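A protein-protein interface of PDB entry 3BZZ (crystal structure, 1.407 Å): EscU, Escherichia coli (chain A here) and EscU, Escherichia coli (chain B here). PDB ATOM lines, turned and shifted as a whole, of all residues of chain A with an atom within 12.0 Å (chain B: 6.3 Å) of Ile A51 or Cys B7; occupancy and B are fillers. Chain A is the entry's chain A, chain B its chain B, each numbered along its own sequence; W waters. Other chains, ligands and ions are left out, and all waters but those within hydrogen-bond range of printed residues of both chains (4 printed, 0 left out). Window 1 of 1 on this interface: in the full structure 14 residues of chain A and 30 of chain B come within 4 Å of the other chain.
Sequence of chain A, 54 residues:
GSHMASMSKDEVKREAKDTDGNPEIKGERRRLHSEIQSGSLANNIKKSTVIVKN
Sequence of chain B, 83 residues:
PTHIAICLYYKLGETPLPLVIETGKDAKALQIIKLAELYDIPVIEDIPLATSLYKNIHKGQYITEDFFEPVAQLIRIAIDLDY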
ATOM      1  N   GLN A  37      10.061  26.207  13.275  1.00  0.00           N
ATOM      2  CA  GLN A  37      10.876  26.465  14.472  1.00  0.00           C
ATOM      3  C   GLN A  37      10.355  27.662  15.260  1.00  0.00           C
ATOM      4  O   GLN A  37       9.723  28.566  14.705  1.00  0.00           O
ATOM      5  CB  GLN A  37      12.361  26.668  14.129  1.00  0.00           C
ATOM      6  CG  GLN A  37      12.727  28.025  13.512  1.00  0.00           C
ATOM      7  CD  GLN A  37      14.100  28.018  12.810  1.00  0.00           C
ATOM      8  OE1 GLN A  37      14.322  27.266  11.855  1.00  0.00           O
ATOM      9  NE2 GLN A  37      15.004  28.882  13.264  1.00  0.00           N
ATOM     10  N   SER A  38      10.629  27.655  16.561  1.00  0.00           N
ATOM     11  CA  SER A  38      10.235  28.760  17.421  1.00  0.00           C
ATOM     12  C   SER A  38      11.175  29.933  17.176  1.00  0.00           C
ATOM     13  O   SER A  38      12.332  29.742  16.791  1.00  0.00           O
ATOM     14  CB  SER A  38      10.336  28.344  18.879  1.00  0.00           C
ATOM     15  OG  SER A  38      11.697  28.205  19.218  1.00  0.00           O
ATOM     16  N   SER A  40      12.819  31.559  19.229  1.00  0.00           N
ATOM     17  CA  SER A  40      13.958  31.566  20.151  1.00  0.00           C
ATOM     18  C   SER A  40      15.046  30.545  19.791  1.00  0.00           C
ATOM     19  O   SER A  40      16.127  30.524  20.389  1.00  0.00           O
ATOM     20  CB  SER A  40      13.459  31.266  21.559  1.00  0.00           C
ATOM     21  OG  SER A  40      12.709  30.066  21.569  1.00  0.00           O
ATOM     22  N   LEU A  41      14.774  29.679  18.827  1.00  0.00           N
ATOM     23  CA  LEU A  41      15.684  28.577  18.558  1.00  0.00           C
ATOM     24  C   LEU A  41      17.072  29.070  18.192  1.00  0.00           C
ATOM     25  O   LEU A  41      18.077  28.607  18.737  1.00  0.00           O
ATOM     26  CB  LEU A  41      15.129  27.661  17.450  1.00  0.00           C
ATOM     27  CG  LEU A  41      15.930  26.397  17.141  1.00  0.00           C
ATOM     28  CD1 LEU A  41      16.022  25.516  18.409  1.00  0.00           C
ATOM     29  CD2 LEU A  41      15.323  25.607  15.981  1.00  0.00           C
ATOM     30  N   ALA A  42      17.147  29.964  17.221  1.00  0.00           N
ATOM     31  CA  ALA A  42      18.438  30.423  16.722  1.00  0.00           C
ATOM     32  C   ALA A  42      19.239  31.112  17.835  1.00  0.00           C
ATOM     33  O   ALA A  42      20.445  30.880  17.972  1.00  0.00           O
ATOM     34  CB  ALA A  42      18.249  31.354  15.518  1.00  0.00           C
ATOM     35  N   ASN A  43      18.566  31.935  18.645  1.00  0.00           N
ATOM     36  CA  ASN A  43      19.247  32.626  19.739  1.00  0.00           C
ATOM     37  C   ASN A  43      19.798  31.634  20.758  1.00  0.00           C
ATOM     38  O   ASN A  43      20.897  31.822  21.277  1.00  0.00           O
ATOM     39  CB  ASN A  43      18.302  33.623  20.440  1.00  0.00           C
ATOM     40  CG  ASN A  43      19.036  34.606  21.358  1.00  0.00           C
ATOM     41  OD1 ASN A  43      19.984  35.279  20.938  1.00  0.00           O
ATOM     42  ND2 ASN A  43      18.569  34.728  22.603  1.00  0.00           N
ATOM     43  N   ASN A  44      19.039  30.582  21.049  1.00  0.00           N
ATOM     44  CA  ASN A  44      19.509  29.558  21.979  1.00  0.00           C
ATOM     45  C   ASN A  44      20.720  28.798  21.447  1.00  0.00           C
ATOM     46  O   ASN A  44      21.661  28.521  22.188  1.00  0.00           O
ATOM     47  CB  ASN A  44      18.391  28.576  22.310  1.00  0.00           C
ATOM     48  CG  ASN A  44      17.352  29.153  23.260  1.00  0.00           C
ATOM     49  OD1 ASN A  44      17.620  30.098  24.010  1.00  0.00           O
ATOM     50  ND2 ASN A  44      16.159  28.564  23.248  1.00  0.00           N
ATOM     51  N   ILE A  45      20.702  28.464  20.158  1.00  0.00           N
ATOM     52  CA  ILE A  45      21.860  27.830  19.541  1.00  0.00           C
ATOM     53  C   ILE A  45      23.093  28.749  19.624  1.00  0.00           C
ATOM     54  O   ILE A  45      24.179  28.315  20.018  1.00  0.00           O
ATOM     55  CB  ILE A  45      21.523  27.419  18.095  1.00  0.00           C
ATOM     56  CG1 ILE A  45      20.451  26.321  18.127  1.00  0.00           C
ATOM     57  CG2 ILE A  45      22.757  26.941  17.367  1.00  0.00           C
ATOM     58  CD1 ILE A  45      19.790  26.034  16.807  1.00  0.00           C
ATOM     59  N   LYS A  46      22.923  30.019  19.279  1.00  0.00           N
ATOM     60  CA  LYS A  46      24.052  30.937  19.237  1.00  0.00           C
ATOM     61  C   LYS A  46      24.672  31.139  20.603  1.00  0.00           C
ATOM     62  O   LYS A  46      25.866  31.444  20.689  1.00  0.00           O
ATOM     63  CB  LYS A  46      23.622  32.277  18.679  1.00  0.00           C
ATOM     64  CG  LYS A  46      23.331  32.207  17.206  1.00  0.00           C
ATOM     65  CD  LYS A  46      22.732  33.512  16.740  1.00  0.00           C
ATOM     66  CE  LYS A  46      22.471  33.551  15.253  1.00  0.00           C
ATOM     67  NZ  LYS A  46      22.010  34.903  14.831  1.00  0.00           N
ATOM     68  N   LYS A  47      23.847  31.028  21.652  1.00  0.00           N
ATOM     69  CA  LYS A  47      24.266  31.160  23.058  1.00  0.00           C
ATOM     70  C   LYS A  47      24.975  29.921  23.588  1.00  0.00           C
ATOM     71  O   LYS A  47      25.668  29.978  24.615  1.00  0.00           O
ATOM     72  CB  LYS A  47      23.012  31.445  23.921  1.00  0.00           C
ATOM     73  CG  LYS A  47      23.197  31.439  25.382  1.00  0.00           C
ATOM     74  CD  LYS A  47      22.007  32.087  26.031  1.00  0.00           C
ATOM     75  CE  LYS A  47      22.289  32.516  27.432  1.00  0.00           C
ATOM     76  NZ  LYS A  47      21.134  33.233  27.987  1.00  0.00           N
ATOM     77  N   SER A  48      24.809  28.796  22.904  1.00  0.00           N
ATOM     78  CA  SER A  48      25.258  27.514  23.438  1.00  0.00           C
ATOM     79  C   SER A  48      26.756  27.402  23.487  1.00  0.00           C
ATOM     80  O   SER A  48      27.472  27.942  22.647  1.00  0.00           O
ATOM     81  CB  SER A  48      24.700  26.361  22.619  1.00  0.00           C
ATOM     82  OG  SER A  48      23.290  26.279  22.750  1.00  0.00           O
ATOM     83  N   THR A  49      27.227  26.692  24.500  1.00  0.00           N
ATOM     84  CA  THR A  49      28.636  26.429  24.668  1.00  0.00           C
ATOM     85  C   THR A  49      29.034  25.211  23.818  1.00  0.00           C
ATOM     86  O   THR A  49      30.082  25.201  23.178  1.00  0.00           O
ATOM     87  CB  THR A  49      28.923  26.141  26.152  1.00  0.00           C
ATOM     88  OG1 THR A  49      28.409  27.225  26.953  1.00  0.00           O
ATOM     89  CG2 THR A  49      30.412  25.950  26.393  1.00  0.00           C
ATOM     90  N   VAL A  50      28.182  24.190  23.826  1.00  0.00           N
ATOM     91  CA  VAL A  50      28.402  22.993  23.022  1.00  0.00           C
ATOM     92  C   VAL A  50      27.068  22.326  22.804  1.00  0.00           C
ATOM     93  O   VAL A  50      26.166  22.423  23.637  1.00  0.00           O
ATOM     94  CB  VAL A  50      29.383  22.023  23.708  1.00  0.00           C
ATOM     95  CG1 VAL A  50      28.815  21.481  25.024  1.00  0.00           C
ATOM     96  CG2 VAL A  50      29.775  20.867  22.774  1.00  0.00           C
ATOM     97  N   ILE A  51      26.952  21.673  21.665  1.00  0.00           N
ATOM     98  CA  ILE A  51      25.795  20.876  21.328  1.00  0.00           C
ATOM     99  C   ILE A  51      26.241  19.426  21.194  1.00  0.00           C
ATOM    100  O   ILE A  51      27.243  19.139  20.559  1.00  0.00           O
ATOM    101  CB  ILE A  51      25.137  21.419  20.074  1.00  0.00           C
ATOM    102  CG1 ILE A  51      24.605  22.829  20.401  1.00  0.00           C
ATOM    103  CG2 ILE A  51      24.058  20.470  19.558  1.00  0.00           C
ATOM    104  CD1 ILE A  51      24.162  23.628  19.260  1.00  0.00           C
ATOM    105  N   VAL A  52      25.505  18.519  21.837  1.00  0.00           N
ATOM    106  CA  VAL A  52      25.831  17.094  21.745  1.00  0.00           C
ATOM    107  C   VAL A  52      24.695  16.394  21.013  1.00  0.00           C
ATOM    108  O   VAL A  52      23.509  16.674  21.260  1.00  0.00           O
ATOM    109  CB  VAL A  52      26.132  16.469  23.111  1.00  0.00           C
ATOM    110  CG1 VAL A  52      24.973  16.477  24.014  1.00  0.00           C
ATOM    111  CG2 VAL A  52      26.660  15.054  22.959  1.00  0.00           C
ATOM    112  N   LYS A  53      25.050  15.547  20.057  1.00  0.00           N
ATOM    113  CA  LYS A  53      24.077  14.831  19.242  1.00  0.00           C
ATOM    114  C   LYS A  53      24.287  13.322  19.285  1.00  0.00           C
ATOM    115  O   LYS A  53      25.370  12.825  19.599  1.00  0.00           O
ATOM    116  CB  LYS A  53      24.120  15.307  17.781  1.00  0.00           C
ATOM    117  CG  LYS A  53      25.407  14.993  17.073  1.00  0.00           C
ATOM    118  CD  LYS A  53      25.374  15.331  15.561  1.00  0.00           C
ATOM    119  CE  LYS A  53      26.597  14.825  14.885  1.00  0.00           C
ATOM    120  NZ  LYS A  53      26.574  15.114  13.391  1.00  0.00           N
ATOM    121  N   ASN A  54      23.241  12.578  18.945  1.00  0.00           N
ATOM    122  CA  ASN A  54      23.373  11.145  18.696  1.00  0.00           C
ATOM    123  C   ASN A  54      23.649  10.915  17.215  1.00  0.00           C
ATOM    124  O   ASN A  54      23.402   9.844  16.632  1.00  0.00           O
ATOM    125  CB  ASN A  54      22.140  10.347  19.173  1.00  0.00           C
ATOM    126  CG  ASN A  54      20.945  10.562  18.311  1.00  0.00           C
ATOM    127  OD1 ASN A  54      20.914  11.495  17.521  1.00  0.00           O
ATOM    128  ND2 ASN A  54      19.949   9.719  18.465  1.00  0.00           N
ATOM    129  OXT ASN A  54      24.178  11.835  16.564  1.00  0.00           O
ATOM    130  N   ALA B   5      19.392  16.228  19.701  1.00  0.00           N
ATOM    131  CA  ALA B   5      20.393  17.299  19.866  1.00  0.00           C
ATOM    132  C   ALA B   5      20.112  17.963  21.198  1.00  0.00           C
ATOM    133  O   ALA B   5      18.970  18.318  21.492  1.00  0.00           O
ATOM    134  CB  ALA B   5      20.336  18.311  18.764  1.00  0.00           C
ATOM    135  N   ILE B   6      21.157  18.124  22.006  1.00  0.00           N
ATOM    136  CA  ILE B   6      21.085  18.801  23.311  1.00  0.00           C
ATOM    137  C   ILE B   6      22.024  19.996  23.291  1.00  0.00           C
ATOM    138  O   ILE B   6      23.217  19.852  23.045  1.00  0.00           O
ATOM    139  CB  ILE B   6      21.536  17.870  24.444  1.00  0.00           C
ATOM    140  CG1 ILE B   6      20.813  16.510  24.419  1.00  0.00           C
ATOM    141  CG2 ILE B   6      21.404  18.553  25.822  1.00  0.00           C
ATOM    142  CD1 ILE B   6      19.365  16.546  24.656  1.00  0.00           C
ATOM    143  N   CYS B   7      21.488  21.169  23.627  1.00  0.00           N
ATOM    144  CA  CYS B   7      22.263  22.404  23.695  1.00  0.00           C
ATOM    145  C   CYS B   7      22.580  22.729  25.127  1.00  0.00           C
ATOM    146  O   CYS B   7      21.672  22.964  25.914  1.00  0.00           O
ATOM    147  CB  CYS B   7      21.475  23.566  23.087  1.00  0.00           C
ATOM    148  SG  CYS B   7      20.994  23.310  21.342  1.00  0.00           S
ATOM    149  N   LEU B   8      23.874  22.748  25.421  1.00  0.00           N
ATOM    150  CA  LEU B   8      24.396  23.002  26.759  1.00  0.00           C
ATOM    151  C   LEU B   8      25.008  24.378  26.840  1.00  0.00           C
ATOM    152  O   LEU B   8      25.735  24.835  25.951  1.00  0.00           O
ATOM    153  CB  LEU B   8      25.459  21.939  27.097  1.00  0.00           C
ATOM    154  CG  LEU B   8      24.852  20.546  27.333  1.00  0.00           C
ATOM    155  CD1 LEU B   8      25.913  19.474  27.040  1.00  0.00           C
ATOM    156  CD2 LEU B   8      24.286  20.403  28.753  1.00  0.00           C
ATOM    157  N   TYR B   9      24.725  25.028  27.966  1.00  0.00           N
ATOM    158  CA  TYR B   9      25.215  26.360  28.253  1.00  0.00           C
ATOM    159  C   TYR B   9      25.907  26.389  29.599  1.00  0.00           C
ATOM    160  O   TYR B   9      25.359  25.935  30.597  1.00  0.00           O
ATOM    161  CB  TYR B   9      24.046  27.347  28.277  1.00  0.00           C
ATOM    162  CG  TYR B   9      24.409  28.753  28.656  1.00  0.00           C
ATOM    163  CD1 TYR B   9      23.966  29.316  29.850  1.00  0.00           C
ATOM    164  CD2 TYR B   9      25.189  29.546  27.820  1.00  0.00           C
ATOM    165  CE1 TYR B   9      24.281  30.601  30.180  1.00  0.00           C
ATOM    166  CE2 TYR B   9      25.517  30.848  28.151  1.00  0.00           C
ATOM    167  CZ  TYR B   9      25.068  31.368  29.350  1.00  0.00           C
ATOM    168  OH  TYR B   9      25.379  32.665  29.705  1.00  0.00           O
ATOM    169  N   LEU B  19      23.834  23.972  31.977  1.00  0.00           N
ATOM    170  CA  LEU B  19      22.401  24.135  31.823  1.00  0.00           C
ATOM    171  C   LEU B  19      21.943  23.658  30.439  1.00  0.00           C
ATOM    172  O   LEU B  19      22.567  24.027  29.448  1.00  0.00           O
ATOM    173  CB  LEU B  19      22.073  25.618  31.980  1.00  0.00           C
ATOM    174  CG  LEU B  19      20.612  26.031  31.883  1.00  0.00           C
ATOM    175  CD1 LEU B  19      19.822  25.454  33.028  1.00  0.00           C
ATOM    176  CD2 LEU B  19      20.528  27.574  31.889  1.00  0.00           C
ATOM    177  N   VAL B  20      20.904  22.826  30.359  1.00  0.00           N
ATOM    178  CA  VAL B  20      20.342  22.476  29.047  1.00  0.00           C
ATOM    179  C   VAL B  20      19.366  23.597  28.669  1.00  0.00           C
ATOM    180  O   VAL B  20      18.375  23.822  29.345  1.00  0.00           O
ATOM    181  CB  VAL B  20      19.644  21.126  29.092  1.00  0.00           C
ATOM    182  CG1 VAL B  20      18.888  20.856  27.768  1.00  0.00           C
ATOM    183  CG2 VAL B  20      20.662  20.012  29.326  1.00  0.00           C
ATOM    184  N   ILE B  21      19.698  24.343  27.626  1.00  0.00           N
ATOM    185  CA  ILE B  21      18.889  25.483  27.213  1.00  0.00           C
ATOM    186  C   ILE B  21      17.979  25.200  26.028  1.00  0.00           C
ATOM    187  O   ILE B  21      17.081  25.977  25.738  1.00  0.00           O
ATOM    188  CB  ILE B  21      19.737  26.760  26.983  1.00  0.00           C
ATOM    189  CG1 ILE B  21      20.726  26.618  25.832  1.00  0.00           C
ATOM    190  CG2 ILE B  21      20.363  27.188  28.335  1.00  0.00           C
ATOM    191  CD1 ILE B  21      21.358  27.972  25.436  1.00  0.00           C
ATOM    192  N   GLU B  22      18.218  24.096  25.339  1.00  0.00           N
ATOM    193  CA  GLU B  22      17.431  23.786  24.163  1.00  0.00           C
ATOM    194  C   GLU B  22      17.661  22.320  23.872  1.00  0.00           C
ATOM    195  O   GLU B  22      18.749  21.784  24.090  1.00  0.00           O
ATOM    196  CB  GLU B  22      17.871  24.627  22.965  1.00  0.00           C
ATOM    197  CG  GLU B  22      17.037  24.493  21.682  1.00  0.00           C
ATOM    198  CD  GLU B  22      15.628  24.947  21.891  1.00  0.00           C
ATOM    199  OE1 GLU B  22      15.358  26.155  21.699  1.00  0.00           O
ATOM    200  OE2 GLU B  22      14.777  24.117  22.288  1.00  0.00           O
ATOM    201  N   THR B  23      16.612  21.655  23.406  1.00  0.00           N
ATOM    202  CA  THR B  23      16.711  20.256  22.997  1.00  0.00           C
ATOM    203  C   THR B  23      15.858  20.042  21.761  1.00  0.00           C
ATOM    204  O   THR B  23      14.967  20.838  21.426  1.00  0.00           O
ATOM    205  CB  THR B  23      16.165  19.328  24.085  1.00  0.00           C
ATOM    206  OG1 THR B  23      14.755  19.543  24.244  1.00  0.00           O
ATOM    207  CG2 THR B  23      16.877  19.548  25.433  1.00  0.00           C
ATOM    208  N   ILE B  32      18.613  21.882  14.679  1.00  0.00           N
ATOM    209  CA  ILE B  32      19.621  22.368  15.637  1.00  0.00           C
ATOM    210  C   ILE B  32      21.024  22.096  15.130  1.00  0.00           C
ATOM    211  O   ILE B  32      21.878  22.977  15.174  1.00  0.00           O
ATOM    212  CB  ILE B  32      19.419  21.742  17.037  1.00  0.00           C
ATOM    213  CG1 ILE B  32      18.158  22.291  17.687  1.00  0.00           C
ATOM    214  CG2 ILE B  32      20.641  22.007  17.926  1.00  0.00           C
ATOM    215  CD1 ILE B  32      17.700  21.454  18.868  1.00  0.00           C
ATOM    216  N   ILE B  33      21.265  20.892  14.631  1.00  0.00           N
ATOM    217  CA  ILE B  33      22.609  20.490  14.188  1.00  0.00           C
ATOM    218  C   ILE B  33      23.047  21.341  12.992  1.00  0.00           C
ATOM    219  O   ILE B  33      24.196  21.781  12.899  1.00  0.00           O
ATOM    220  CB  ILE B  33      22.663  18.961  13.877  1.00  0.00           C
ATOM    221  CG1 ILE B  33      22.420  18.195  15.192  1.00  0.00           C
ATOM    222  CG2 ILE B  33      23.976  18.564  13.165  1.00  0.00           C
ATOM    223  CD1 ILE B  33      21.855  16.823  14.954  1.00  0.00           C
ATOM    224  N   ALA B  36      23.618  24.979  14.137  1.00  0.00           N
ATOM    225  CA  ALA B  36      24.869  25.034  14.907  1.00  0.00           C
ATOM    226  C   ALA B  36      26.086  25.223  14.018  1.00  0.00           C
ATOM    227  O   ALA B  36      26.973  26.048  14.287  1.00  0.00           O
ATOM    228  CB  ALA B  36      25.024  23.779  15.769  1.00  0.00           C
ATOM    229  N   ILE B  41      28.942  26.897  16.226  1.00  0.00           N
ATOM    230  CA  ILE B  41      28.823  26.349  17.576  1.00  0.00           C
ATOM    231  C   ILE B  41      29.318  24.914  17.528  1.00  0.00           C
ATOM    232  O   ILE B  41      28.862  24.134  16.683  1.00  0.00           O
ATOM    233  CB  ILE B  41      27.358  26.339  18.058  1.00  0.00           C
ATOM    234  CG1 ILE B  41      26.754  27.744  17.953  1.00  0.00           C
ATOM    235  CG2 ILE B  41      27.237  25.755  19.502  1.00  0.00           C
ATOM    236  CD1 ILE B  41      27.492  28.801  18.779  1.00  0.00           C
ATOM    237  N   PRO B  42      30.221  24.532  18.436  1.00  0.00           N
ATOM    238  CA  PRO B  42      30.742  23.155  18.400  1.00  0.00           C
ATOM    239  C   PRO B  42      29.646  22.099  18.582  1.00  0.00           C
ATOM    240  O   PRO B  42      28.796  22.235  19.455  1.00  0.00           O
ATOM    241  CB  PRO B  42      31.743  23.122  19.568  1.00  0.00           C
ATOM    242  CG  PRO B  42      32.019  24.504  19.891  1.00  0.00           C
ATOM    243  CD  PRO B  42      30.837  25.319  19.515  1.00  0.00           C
ATOM    244  N   VAL B  43      29.668  21.083  17.728  1.00  0.00           N
ATOM    245  CA  VAL B  43      28.755  19.965  17.795  1.00  0.00           C
ATOM    246  C   VAL B  43      29.594  18.705  17.971  1.00  0.00           C
ATOM    247  O   VAL B  43      30.471  18.433  17.155  1.00  0.00           O
ATOM    248  CB  VAL B  43      27.904  19.847  16.518  1.00  0.00           C
ATOM    249  CG1 VAL B  43      27.040  18.590  16.601  1.00  0.00           C
ATOM    250  CG2 VAL B  43      27.043  21.119  16.324  1.00  0.00           C
ATOM    251  N   ILE B  44      29.307  17.946  19.021  1.00  0.00           N
ATOM    252  CA  ILE B  44      30.016  16.691  19.297  1.00  0.00           C
ATOM    253  C   ILE B  44      29.039  15.528  19.184  1.00  0.00           C
ATOM    254  O   ILE B  44      27.973  15.544  19.773  1.00  0.00           O
ATOM    255  CB  ILE B  44      30.662  16.742  20.705  1.00  0.00           C
ATOM    256  CG1 ILE B  44      31.685  17.882  20.752  1.00  0.00           C
ATOM    257  CG2 ILE B  44      31.341  15.415  21.073  1.00  0.00           C
ATOM    258  CD1 ILE B  44      32.476  17.983  22.015  1.00  0.00           C
ATOM    259  N   GLU B  45      29.444  14.493  18.441  1.00  0.00           N
ATOM    260  CA  GLU B  45      28.697  13.257  18.363  1.00  0.00           C
ATOM    261  C   GLU B  45      29.081  12.393  19.553  1.00  0.00           C
ATOM    262  O   GLU B  45      30.248  11.989  19.675  1.00  0.00           O
ATOM    263  CB  GLU B  45      29.025  12.548  17.066  1.00  0.00           C
ATOM    264  CG  GLU B  45      28.233  11.275  16.847  1.00  0.00           C
ATOM    265  CD  GLU B  45      28.562  10.606  15.534  1.00  0.00           C
ATOM    266  OE1 GLU B  45      27.900  10.944  14.528  1.00  0.00           O
ATOM    267  OE2 GLU B  45      29.456   9.770  15.467  1.00  0.00           O
ATOM    268  N   LEU B  74      33.115  16.996  27.916  1.00  0.00           N
ATOM    269  CA  LEU B  74      32.552  17.466  26.660  1.00  0.00           C
ATOM    270  C   LEU B  74      32.861  18.951  26.451  1.00  0.00           C
ATOM    271  O   LEU B  74      33.289  19.371  25.372  1.00  0.00           O
ATOM    272  CB  LEU B  74      31.039  17.264  26.708  1.00  0.00           C
ATOM    273  CG  LEU B  74      30.198  17.556  25.478  1.00  0.00           C
ATOM    274  CD1 LEU B  74      30.394  16.451  24.503  1.00  0.00           C
ATOM    275  CD2 LEU B  74      28.705  17.656  25.851  1.00  0.00           C
HETATM  276  O   HOH W   1      22.578  34.407  30.126  1.00  0.00           O
HETATM  277  O   HOH W   2      25.266  11.202  14.268  1.00  0.00           O
HETATM  278  O   HOH W   3      28.869  13.424  12.949  1.00  0.00           O
HETATM  279  O   HOH W   4      13.061  26.825  20.677  1.00  0.00           O
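The backbone carbonyl oxygen of Ile B44 is in hydrogen-bond range of the backbone NH of Lys A53 (2.9 Å). The backbone carbonyl oxygen of Pro B42 sits at hydrogen-bond distance from the backbone NH of Ile A51 (2.9 Å). The backbone carbonyl oxygen of Val A50 sits at hydrogen-bond distance from the backbone NH of Leu B8 (2.9 Å). The backbone carbonyl oxygen (O) of Val A52 sits at hydrogen-bond distance from the backbone NH (N) of Ile B6. The side-chain amide nitrogen of Asn A44 lies within hydrogen-bond range of the side-chain carboxylate of Glu B22, at 3.0 Å. The backbone carbonyl oxygen (O) of Ile A51 lies within hydrogen-bond range of the backbone NH (N) of Ile B44, at 2.8 Å. N of Thr A49 sits at hydrogen-bond distance from O of Leu B8.
Printed residues of chain B within 4 Å of Ser A48: Cys B7, Leu B8, Ile B21 and Ile B41. Printed residues of chain B within 4 Å of Thr A49: Leu B8, Tyr B9 and Pro B42. Ala B5 touches one residue of chain A. Of chain A, only Val A50 (3.96 Å), Ile A51 (3.3 Å) and Val A52 (2.9 Å) come within 4 Å of Ile B6. Cys B7 touches three residues of chain A. Leu B8 touches just these residues of chain A: Ser A48 (3.7 Å), Thr A49 (2.8 Å) and Val A50 (2.9 Å). No residue of chain A comes within 4 Å of Val B20. Of chain A, only Asn A44 (3.3 Å), Lys A47 (3.9 Å) and Ser A48 (3.7 Å) come within 4 Å of Ile B21. Ile B32 touches two residues of chain A. Ile B33 touches just one residue of chain A: Lys A53 (3.9 Å). Of the printed residues of chain A, Ala B36 touches Ile A45 and Ile A51. Of the printed residues of chain A, Ile B41 touches Ile A45, Lys A46, Ser A48 and Ile A51. Val B43 touches just these residues of chain A: Ile A51 and Lys A53.
N of Ile B41 lies within hydrogen-bond range of O of Ala B36 (2.9 Å). The backbone carbonyl oxygen (O) of Asn A44 is in hydrogen-bond range of the side-chain hydroxyl (OG) of Ser A48 (2.8 Å). N of Cys B7 lies within hydrogen-bond range of O of Glu B22. The backbone carbonyl oxygen (O) of Cys B7 lies within hydrogen-bond range of the backbone NH (N) of Ile B21, at 3.0 Å. ND2 of Asn A44 sits close to O of Ser A40 (3.5 Å). The side-chain hydroxyl of Ser A38 sits at hydrogen-bond distance from the backbone NH of Leu A41, 3.4 Å away.
Of the 19 printed residues of chain B, 16 touch a printed residue of chain A. Printed residues of chain B that touch a printed residue of chain A: Ala B5, Ile B6, Cys B7, Leu B8, Tyr B9, Ile B21, Glu B22, Ile B32, Ile B33, Ala B36, Ile B41, Pro B42, Val B43, Ile B44, Glu B45 and Leu B74. Of the 17 printed residues of chain A, 11 touch a printed residue of chain B. Printed residues of chain A that touch a printed residue of chain B: Leu A41, Asn A44, Ile A45, Lys A46, Lys A47, Ser A48, Thr A49, Val A50, Ile A51, Val A52 and Lys A53. Hydrophobic or aromatic side chains of chain A within 4 Å of the printed part of chain B: Leu A41, Ile A45, Val A50, Ile A51 and Val A52. Among the printed residues, 37 pairs touch across the chains. Among the printed residues, no Asp or Glu carboxylate lies within 4 Å of a Lys or Arg side-chain nitrogen of the other chain.
Among the printed residues, merely in contact across the chains: Leu A41 with Glu B22 (3.4 Å), Leu A41 with Ile B32 (3.9 Å), Asn A44 with Ile B21 (3.3 Å), Ile A45 with Ile B32 (3.9 Å), Ile A45 with Ala B36 (3.8 Å), Ile A45 with Ile B41 (3.3 Å), Lys A46 with Ile B41 (3.6 Å), Lys A47 with Tyr B9 (3.3 Å), Lys A47 with Ile B21 (3.9 Å), Ser A48 with Cys B7 (3.3 Å), Ser A48 with Leu B8 (3.7 Å), Ser A48 with Ile B21 (3.7 Å), Ser A48 with Ile B41 (3.8 Å), Thr A49 with Tyr B9 (3.6 Å), Thr A49 with Pro B42 (3.7 Å), Val A50 with Ile B6 (3.96 Å), Val A50 with Cys B7 (3.9 Å), Val A50 with Pro B42 (3.7 Å), Val A50 with Leu B74 (3.9 Å), Ile A51 with Ile B6 (3.3 Å), Ile A51 with Cys B7 (3.8 Å), Ile A51 with Ala B36 (3.6 Å), Ile A51 with Ile B41 (3.7 Å), Ile A51 with Val B43 (3.3 Å), Val A52 with Ala B5 (3.5 Å), Val A52 with Ile B44 (3.3 Å), Val A52 with Leu B74 (3.9 Å), Lys A53 with Ile B33 (3.9 Å), Lys A53 with Val B43 (3.8 Å) and Lys A53 with Glu B45 (3.6 Å).
Water W4 lies within hydrogen-bond range of the side-chain hydroxyl of Ser A38 (2.4 Å), the side-chain carboxylate of Glu B22 (2.6 Å) and the side-chain hydroxyl of Ser A40 (3.4 Å). Water W2 bridges the chain-end carboxylate of Asn A54 and the side-chain carboxylate of Glu B45. Water W1 bridges NZ of Lys A47 and OH of Tyr B9. Water W3 bridges NZ of Lys A53 (2.9 Å) and OE1 of Glu B45 (3.1 Å).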
